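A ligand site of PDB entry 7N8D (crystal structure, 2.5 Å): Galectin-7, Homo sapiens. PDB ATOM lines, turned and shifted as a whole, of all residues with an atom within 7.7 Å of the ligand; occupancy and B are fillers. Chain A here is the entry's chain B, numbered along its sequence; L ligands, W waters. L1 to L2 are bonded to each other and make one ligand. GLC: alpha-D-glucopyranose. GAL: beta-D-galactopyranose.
The side-chain carboxylate (OE1) of Glu 72 is in salt-bridge range of the guanidinium group (NH1) of Arg 74 (2.9 Å). The side-chain carboxylate (OE2) of Glu 58 is in salt-bridge range of the guanidinium group (NH1) of Arg 53 (3.1 Å). NE of Arg 74 is in salt-bridge range of OE1 of Glu 58, 2.8 Å away. The backbone carbonyl oxygen of Val 60 is in hydrogen-bond range of the backbone NH of Asn 51 (2.9 Å). The backbone NH of His 49 sits at hydrogen-bond distance from the backbone carbonyl oxygen of Asn 62. OD1 of Asn 51 lies within hydrogen-bond range of NE of Arg 53 (2.6 Å). The backbone carbonyl oxygen (O) of Gly 70 is in hydrogen-bond range of the side-chain amide nitrogen (ND2) of Asn 62. The side-chain amide oxygen (OD1) of Asn 62 sits close to the backbone carbonyl oxygen (O) of Arg 71 (2.9 Å).
Water W2 bridges O4 of GLC L1 (2.5 Å) and NH1 of Arg 31 (3.2 Å). Water W3 bridges an oxygen (O2) of GLC L1 (2.8 Å) and the guanidinium group of Arg 74 (3.4 Å). Water W1 bridges the side-chain carboxylate of Glu 72 (3.2 Å) and an oxygen (O6) of GLC L1 (3.5 Å).
An oxygen (O3) of GLC L1 lies within hydrogen-bond range of the side-chain carboxylate (OE2) of Glu 72 (2.7 Å). A ring nitrogen (NE2) of His 49 sits at hydrogen-bond distance from an oxygen (O4) of GAL L2 (3.1 Å). The guanidinium group of Arg 74 sits at hydrogen-bond distance from an oxygen (O2) of GLC L1 (3.4 Å). The side-chain amide oxygen of Asn 51 is in hydrogen-bond range of an oxygen (O4) of GAL L2 (3.1 Å). NH1 of Arg 53 lies within hydrogen-bond range of O3 of GLC L1.
CG1 of Val 60 touches O6 of GAL L2, 3.3 Å away. Asn 62 touches the ligand. CZ2 of Trp 69 touches C4 of GAL L2, 3.6 Å away. Hydrophobic or aromatic side chains within 4 Å of the ligand: His 49, Val 60 and Trp 69. Of the 21 residues printed, 8 come within 4 Å of the ligand.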
ATOM      1  N   ARG A  31     -15.922 -17.539  21.359  1.00  0.00           N
ATOM      2  CA  ARG A  31     -16.539 -18.849  21.312  1.00  0.00           C
ATOM      3  C   ARG A  31     -16.095 -19.585  20.063  1.00  0.00           C
ATOM      4  O   ARG A  31     -15.723 -18.972  19.056  1.00  0.00           O
ATOM      5  CB  ARG A  31     -18.073 -18.745  21.304  1.00  0.00           C
ATOM      6  CG  ARG A  31     -18.617 -17.615  22.159  1.00  0.00           C
ATOM      7  CD  ARG A  31     -20.121 -17.593  22.179  1.00  0.00           C
ATOM      8  NE  ARG A  31     -20.615 -16.998  23.419  1.00  0.00           N
ATOM      9  CZ  ARG A  31     -21.905 -16.929  23.758  1.00  0.00           C
ATOM     10  NH1 ARG A  31     -22.837 -17.411  22.949  1.00  0.00           N
ATOM     11  NH2 ARG A  31     -22.249 -16.361  24.906  1.00  0.00           N
ATOM     12  N   HIS A  33     -17.351 -23.629  18.078  1.00  0.00           N
ATOM     13  CA  HIS A  33     -18.445 -24.591  18.099  1.00  0.00           C
ATOM     14  C   HIS A  33     -18.103 -25.818  17.272  1.00  0.00           C
ATOM     15  O   HIS A  33     -17.334 -25.747  16.314  1.00  0.00           O
ATOM     16  CB  HIS A  33     -19.751 -23.957  17.573  1.00  0.00           C
ATOM     17  CG  HIS A  33     -19.587 -23.217  16.284  1.00  0.00           C
ATOM     18  ND1 HIS A  33     -19.303 -21.876  16.213  1.00  0.00           N
ATOM     19  CD2 HIS A  33     -19.675 -23.649  14.995  1.00  0.00           C
ATOM     20  CE1 HIS A  33     -19.220 -21.503  14.952  1.00  0.00           C
ATOM     21  NE2 HIS A  33     -19.440 -22.563  14.193  1.00  0.00           N
ATOM     22  N   ASN A  35     -20.511 -28.915  15.503  1.00  0.00           N
ATOM     23  CA  ASN A  35     -21.894 -29.250  15.206  1.00  0.00           C
ATOM     24  C   ASN A  35     -21.966 -30.567  14.450  1.00  0.00           C
ATOM     25  O   ASN A  35     -21.149 -30.835  13.560  1.00  0.00           O
ATOM     26  CB  ASN A  35     -22.572 -28.152  14.378  1.00  0.00           C
ATOM     27  CG  ASN A  35     -22.525 -26.796  15.063  1.00  0.00           C
ATOM     28  OD1 ASN A  35     -22.529 -26.712  16.293  1.00  0.00           O
ATOM     29  ND2 ASN A  35     -22.472 -25.732  14.271  1.00  0.00           N
ATOM     30  N   HIS A  49     -24.500 -29.941  19.543  1.00  0.00           N
ATOM     31  CA  HIS A  49     -23.947 -28.597  19.387  1.00  0.00           C
ATOM     32  C   HIS A  49     -23.044 -28.356  20.596  1.00  0.00           C
ATOM     33  O   HIS A  49     -23.531 -28.110  21.704  1.00  0.00           O
ATOM     34  CB  HIS A  49     -25.051 -27.552  19.290  1.00  0.00           C
ATOM     35  CG  HIS A  49     -24.563 -26.141  19.411  1.00  0.00           C
ATOM     36  ND1 HIS A  49     -24.082 -25.420  18.337  1.00  0.00           N
ATOM     37  CD2 HIS A  49     -24.491 -25.313  20.475  1.00  0.00           C
ATOM     38  CE1 HIS A  49     -23.728 -24.218  18.731  1.00  0.00           C
ATOM     39  NE2 HIS A  49     -23.972 -24.125  20.028  1.00  0.00           N
ATOM     40  N   PHE A  50     -21.732 -28.445  20.367  1.00  0.00           N
ATOM     41  CA  PHE A  50     -20.717 -28.358  21.413  1.00  0.00           C
ATOM     42  C   PHE A  50     -20.084 -26.966  21.337  1.00  0.00           C
ATOM     43  O   PHE A  50     -19.299 -26.680  20.433  1.00  0.00           O
ATOM     44  CB  PHE A  50     -19.685 -29.471  21.230  1.00  0.00           C
ATOM     45  CG  PHE A  50     -18.521 -29.411  22.184  1.00  0.00           C
ATOM     46  CD1 PHE A  50     -18.660 -29.858  23.486  1.00  0.00           C
ATOM     47  CD2 PHE A  50     -17.296 -28.935  21.764  1.00  0.00           C
ATOM     48  CE1 PHE A  50     -17.585 -29.806  24.354  1.00  0.00           C
ATOM     49  CE2 PHE A  50     -16.230 -28.888  22.630  1.00  0.00           C
ATOM     50  CZ  PHE A  50     -16.373 -29.327  23.931  1.00  0.00           C
ATOM     51  N   ASN A  51     -20.415 -26.111  22.313  1.00  0.00           N
ATOM     52  CA  ASN A  51     -20.160 -24.671  22.233  1.00  0.00           C
ATOM     53  C   ASN A  51     -19.348 -24.192  23.432  1.00  0.00           C
ATOM     54  O   ASN A  51     -19.902 -23.688  24.417  1.00  0.00           O
ATOM     55  CB  ASN A  51     -21.496 -23.916  22.135  1.00  0.00           C
ATOM     56  CG  ASN A  51     -21.312 -22.421  21.911  1.00  0.00           C
ATOM     57  OD1 ASN A  51     -22.177 -21.621  22.294  1.00  0.00           O
ATOM     58  ND2 ASN A  51     -20.203 -22.030  21.287  1.00  0.00           N
ATOM     59  N   ARG A  53     -17.157 -21.466  25.358  1.00  0.00           N
ATOM     60  CA  ARG A  53     -17.310 -20.010  25.396  1.00  0.00           C
ATOM     61  C   ARG A  53     -16.286 -19.433  26.362  1.00  0.00           C
ATOM     62  O   ARG A  53     -16.427 -19.581  27.580  1.00  0.00           O
ATOM     63  CB  ARG A  53     -18.729 -19.631  25.820  1.00  0.00           C
ATOM     64  CG  ARG A  53     -19.826 -20.071  24.862  1.00  0.00           C
ATOM     65  CD  ARG A  53     -21.198 -19.906  25.490  1.00  0.00           C
ATOM     66  NE  ARG A  53     -22.273 -20.363  24.610  1.00  0.00           N
ATOM     67  CZ  ARG A  53     -23.557 -20.320  24.923  1.00  0.00           C
ATOM     68  NH1 ARG A  53     -23.949 -19.839  26.096  1.00  0.00           N
ATOM     69  NH2 ARG A  53     -24.463 -20.755  24.060  1.00  0.00           N
ATOM     70  N   THR A  56     -18.063 -15.998  28.352  1.00  0.00           N
ATOM     71  CA  THR A  56     -18.929 -16.245  29.493  1.00  0.00           C
ATOM     72  C   THR A  56     -18.471 -17.442  30.325  1.00  0.00           C
ATOM     73  O   THR A  56     -19.200 -17.875  31.220  1.00  0.00           O
ATOM     74  CB  THR A  56     -20.368 -16.442  29.032  1.00  0.00           C
ATOM     75  OG1 THR A  56     -20.459 -17.598  28.176  1.00  0.00           O
ATOM     76  CG2 THR A  56     -20.864 -15.211  28.280  1.00  0.00           C
ATOM     77  N   GLU A  58     -18.001 -20.908  29.980  1.00  0.00           N
ATOM     78  CA  GLU A  58     -18.906 -22.046  30.061  1.00  0.00           C
ATOM     79  C   GLU A  58     -18.793 -22.884  28.807  1.00  0.00           C
ATOM     80  O   GLU A  58     -18.272 -22.440  27.780  1.00  0.00           O
ATOM     81  CB  GLU A  58     -20.350 -21.601  30.287  1.00  0.00           C
ATOM     82  CG  GLU A  58     -20.839 -20.566  29.277  1.00  0.00           C
ATOM     83  CD  GLU A  58     -22.264 -20.123  29.547  1.00  0.00           C
ATOM     84  OE1 GLU A  58     -22.894 -20.682  30.468  1.00  0.00           O
ATOM     85  OE2 GLU A  58     -22.753 -19.212  28.832  1.00  0.00           O
ATOM     86  N   VAL A  59     -19.301 -24.107  28.891  1.00  0.00           N
ATOM     87  CA  VAL A  59     -19.378 -25.043  27.770  1.00  0.00           C
ATOM     88  C   VAL A  59     -20.813 -25.537  27.692  1.00  0.00           C
ATOM     89  O   VAL A  59     -21.293 -26.189  28.623  1.00  0.00           O
ATOM     90  CB  VAL A  59     -18.395 -26.215  27.925  1.00  0.00           C
ATOM     91  CG1 VAL A  59     -18.477 -27.149  26.731  1.00  0.00           C
ATOM     92  CG2 VAL A  59     -16.977 -25.713  28.123  1.00  0.00           C
ATOM     93  N   VAL A  60     -21.488 -25.225  26.589  1.00  0.00           N
ATOM     94  CA  VAL A  60     -22.905 -25.523  26.424  1.00  0.00           C
ATOM     95  C   VAL A  60     -23.067 -26.667  25.430  1.00  0.00           C
ATOM     96  O   VAL A  60     -22.393 -26.700  24.388  1.00  0.00           O
ATOM     97  CB  VAL A  60     -23.688 -24.278  25.956  1.00  0.00           C
ATOM     98  CG1 VAL A  60     -25.163 -24.607  25.743  1.00  0.00           C
ATOM     99  CG2 VAL A  60     -23.532 -23.147  26.960  1.00  0.00           C
ATOM    100  N   PHE A  61     -23.961 -27.594  25.750  1.00  0.00           N
ATOM    101  CA  PHE A  61     -24.392 -28.658  24.850  1.00  0.00           C
ATOM    102  C   PHE A  61     -25.879 -28.458  24.569  1.00  0.00           C
ATOM    103  O   PHE A  61     -26.632 -28.032  25.458  1.00  0.00           O
ATOM    104  CB  PHE A  61     -24.193 -30.051  25.458  1.00  0.00           C
ATOM    105  CG  PHE A  61     -22.765 -30.355  25.856  1.00  0.00           C
ATOM    106  CD1 PHE A  61     -22.168 -29.677  26.905  1.00  0.00           C
ATOM    107  CD2 PHE A  61     -22.048 -31.338  25.206  1.00  0.00           C
ATOM    108  CE1 PHE A  61     -20.863 -29.959  27.277  1.00  0.00           C
ATOM    109  CE2 PHE A  61     -20.750 -31.626  25.568  1.00  0.00           C
ATOM    110  CZ  PHE A  61     -20.157 -30.939  26.614  1.00  0.00           C
ATOM    111  N   ASN A  62     -26.312 -28.749  23.351  1.00  0.00           N
ATOM    112  CA  ASN A  62     -27.727 -28.570  23.025  1.00  0.00           C
ATOM    113  C   ASN A  62     -28.059 -29.267  21.720  1.00  0.00           C
ATOM    114  O   ASN A  62     -27.178 -29.729  20.983  1.00  0.00           O
ATOM    115  CB  ASN A  62     -28.092 -27.077  22.947  1.00  0.00           C
ATOM    116  CG  ASN A  62     -29.508 -26.810  23.377  1.00  0.00           C
ATOM    117  OD1 ASN A  62     -30.329 -27.722  23.462  1.00  0.00           O
ATOM    118  ND2 ASN A  62     -29.813 -25.545  23.662  1.00  0.00           N
ATOM    119  N   SER A  63     -29.366 -29.320  21.437  1.00  0.00           N
ATOM    120  CA  SER A  63     -29.903 -29.885  20.208  1.00  0.00           C
ATOM    121  C   SER A  63     -30.902 -28.893  19.614  1.00  0.00           C
ATOM    122  O   SER A  63     -31.564 -28.160  20.352  1.00  0.00           O
ATOM    123  CB  SER A  63     -30.620 -31.218  20.466  1.00  0.00           C
ATOM    124  OG  SER A  63     -31.874 -30.995  21.087  1.00  0.00           O
ATOM    125  N   LYS A  64     -30.956 -28.804  18.277  1.00  0.00           N
ATOM    126  CA  LYS A  64     -31.900 -27.909  17.543  1.00  0.00           C
ATOM    127  C   LYS A  64     -32.869 -28.817  16.758  1.00  0.00           C
ATOM    128  O   LYS A  64     -32.421 -29.863  16.273  1.00  0.00           O
ATOM    129  CB  LYS A  64     -31.199 -26.887  16.640  1.00  0.00           C
ATOM    130  CG  LYS A  64     -32.029 -25.640  16.276  1.00  0.00           C
ATOM    131  CD  LYS A  64     -31.402 -24.771  15.125  1.00  0.00           C
ATOM    132  CE  LYS A  64     -30.165 -23.974  15.554  1.00  0.00           C
ATOM    133  NZ  LYS A  64     -29.455 -23.343  14.381  1.00  0.00           N
ATOM    134  N   TRP A  69     -34.007 -24.289  19.569  1.00  0.00           N
ATOM    135  CA  TRP A  69     -33.033 -24.888  20.471  1.00  0.00           C
ATOM    136  C   TRP A  69     -33.738 -25.683  21.566  1.00  0.00           C
ATOM    137  O   TRP A  69     -34.897 -25.434  21.903  1.00  0.00           O
ATOM    138  CB  TRP A  69     -32.171 -23.793  21.117  1.00  0.00           C
ATOM    139  CG  TRP A  69     -31.174 -23.191  20.175  1.00  0.00           C
ATOM    140  CD1 TRP A  69     -31.237 -21.951  19.593  1.00  0.00           C
ATOM    141  CD2 TRP A  69     -29.964 -23.790  19.703  1.00  0.00           C
ATOM    142  NE1 TRP A  69     -30.144 -21.749  18.789  1.00  0.00           N
ATOM    143  CE2 TRP A  69     -29.340 -22.865  18.841  1.00  0.00           C
ATOM    144  CE3 TRP A  69     -29.341 -25.026  19.925  1.00  0.00           C
ATOM    145  CZ2 TRP A  69     -28.140 -23.132  18.196  1.00  0.00           C
ATOM    146  CZ3 TRP A  69     -28.147 -25.283  19.287  1.00  0.00           C
ATOM    147  CH2 TRP A  69     -27.553 -24.347  18.439  1.00  0.00           C
ATOM    148  N   GLY A  70     -33.025 -26.661  22.105  1.00  0.00           N
ATOM    149  CA  GLY A  70     -33.534 -27.517  23.153  1.00  0.00           C
ATOM    150  C   GLY A  70     -33.038 -27.099  24.529  1.00  0.00           C
ATOM    151  O   GLY A  70     -32.625 -25.953  24.756  1.00  0.00           O
ATOM    152  N   ARG A  71     -33.101 -28.043  25.465  1.00  0.00           N
ATOM    153  CA  ARG A  71     -32.594 -27.788  26.805  1.00  0.00           C
ATOM    154  C   ARG A  71     -31.068 -27.720  26.777  1.00  0.00           C
ATOM    155  O   ARG A  71     -30.407 -28.590  26.192  1.00  0.00           O
ATOM    156  CB  ARG A  71     -33.057 -28.883  27.762  1.00  0.00           C
ATOM    157  CG  ARG A  71     -32.548 -28.733  29.189  1.00  0.00           C
ATOM    158  CD  ARG A  71     -33.022 -29.860  30.087  1.00  0.00           C
ATOM    159  NE  ARG A  71     -34.481 -29.848  30.260  1.00  0.00           N
ATOM    160  CZ  ARG A  71     -35.152 -30.739  30.975  1.00  0.00           C
ATOM    161  NH1 ARG A  71     -34.519 -31.729  31.584  1.00  0.00           N
ATOM    162  NH2 ARG A  71     -36.475 -30.643  31.068  1.00  0.00           N
ATOM    163  N   GLU A  72     -30.508 -26.699  27.419  1.00  0.00           N
ATOM    164  CA  GLU A  72     -29.073 -26.515  27.450  1.00  0.00           C
ATOM    165  C   GLU A  72     -28.462 -27.333  28.585  1.00  0.00           C
ATOM    166  O   GLU A  72     -28.949 -27.287  29.721  1.00  0.00           O
ATOM    167  CB  GLU A  72     -28.720 -25.033  27.628  1.00  0.00           C
ATOM    168  CG  GLU A  72     -29.031 -24.185  26.411  1.00  0.00           C
ATOM    169  CD  GLU A  72     -28.531 -22.760  26.563  1.00  0.00           C
ATOM    170  OE1 GLU A  72     -28.404 -22.286  27.709  1.00  0.00           O
ATOM    171  OE2 GLU A  72     -28.269 -22.106  25.530  1.00  0.00           O
ATOM    172  N   GLU A  73     -27.403 -28.064  28.268  1.00  0.00           N
ATOM    173  CA  GLU A  73     -26.599 -28.786  29.250  1.00  0.00           C
ATOM    174  C   GLU A  73     -25.241 -28.109  29.349  1.00  0.00           C
ATOM    175  O   GLU A  73     -24.676 -27.686  28.333  1.00  0.00           O
ATOM    176  CB  GLU A  73     -26.447 -30.257  28.864  1.00  0.00           C
ATOM    177  CG  GLU A  73     -27.764 -30.993  28.669  1.00  0.00           C
ATOM    178  CD  GLU A  73     -27.594 -32.490  28.568  1.00  0.00           C
ATOM    179  OE1 GLU A  73     -26.453 -32.981  28.745  1.00  0.00           O
ATOM    180  OE2 GLU A  73     -28.590 -33.195  28.303  1.00  0.00           O
ATOM    181  N   ARG A  74     -24.726 -28.016  30.570  1.00  0.00           N
ATOM    182  CA  ARG A  74     -23.457 -27.332  30.837  1.00  0.00           C
ATOM    183  C   ARG A  74     -22.479 -28.296  31.494  1.00  0.00           C
ATOM    184  O   ARG A  74     -22.837 -29.025  32.418  1.00  0.00           O
ATOM    185  CB  ARG A  74     -23.668 -26.106  31.719  1.00  0.00           C
ATOM    186  CG  ARG A  74     -23.763 -24.791  30.946  1.00  0.00           C
ATOM    187  CD  ARG A  74     -24.674 -23.792  31.640  1.00  0.00           C
ATOM    188  NE  ARG A  74     -24.868 -22.588  30.855  1.00  0.00           N
ATOM    189  CZ  ARG A  74     -25.884 -22.372  30.021  1.00  0.00           C
ATOM    190  NH1 ARG A  74     -26.824 -23.289  29.859  1.00  0.00           N
ATOM    191  NH2 ARG A  74     -25.956 -21.228  29.349  1.00  0.00           N
HETATM  192  C1  GLC L   1     -30.011 -18.208  26.689  1.00  0.00           C
HETATM  193  C2  GLC L   1     -28.778 -19.099  26.726  1.00  0.00           C
HETATM  194  C3  GLC L   1     -27.778 -18.761  25.679  1.00  0.00           C
HETATM  195  C4  GLC L   1     -28.398 -18.630  24.325  1.00  0.00           C
HETATM  196  C5  GLC L   1     -29.524 -17.588  24.357  1.00  0.00           C
HETATM  197  C6  GLC L   1     -30.140 -17.444  23.002  1.00  0.00           C
HETATM  198  O1  GLC L   1     -29.690 -16.992  27.219  1.00  0.00           O
HETATM  199  O2  GLC L   1     -28.159 -18.959  28.021  1.00  0.00           O
HETATM  200  O3  GLC L   1     -26.774 -19.807  25.645  1.00  0.00           O
HETATM  201  O4  GLC L   1     -27.380 -18.259  23.379  1.00  0.00           O
HETATM  202  O5  GLC L   1     -30.564 -18.004  25.306  1.00  0.00           O
HETATM  203  O6  GLC L   1     -30.630 -18.680  22.557  1.00  0.00           O
HETATM  204  C1  GAL L   2     -27.439 -19.113  22.322  1.00  0.00           C
HETATM  205  C2  GAL L   2     -26.330 -18.815  21.311  1.00  0.00           C
HETATM  206  C3  GAL L   2     -26.412 -19.758  20.169  1.00  0.00           C
HETATM  207  C4  GAL L   2     -26.408 -21.184  20.623  1.00  0.00           C
HETATM  208  C5  GAL L   2     -27.455 -21.460  21.694  1.00  0.00           C
HETATM  209  C6  GAL L   2     -27.296 -22.847  22.222  1.00  0.00           C
HETATM  210  O2  GAL L   2     -26.461 -17.470  20.835  1.00  0.00           O
HETATM  211  O3  GAL L   2     -25.277 -19.555  19.280  1.00  0.00           O
HETATM  212  O4  GAL L   2     -25.117 -21.475  21.179  1.00  0.00           O
HETATM  213  O5  GAL L   2     -27.323 -20.519  22.814  1.00  0.00           O
HETATM  214  O6  GAL L   2     -26.235 -22.862  23.127  1.00  0.00           O
HETATM  215  O   HOH W   1     -30.858 -21.924  23.715  1.00  0.00           O
HETATM  216  O   HOH W   2     -25.768 -16.341  23.766  1.00  0.00           O
HETATM  217  O   HOH W   3     -28.313 -19.307  30.785  1.00  0.00           O
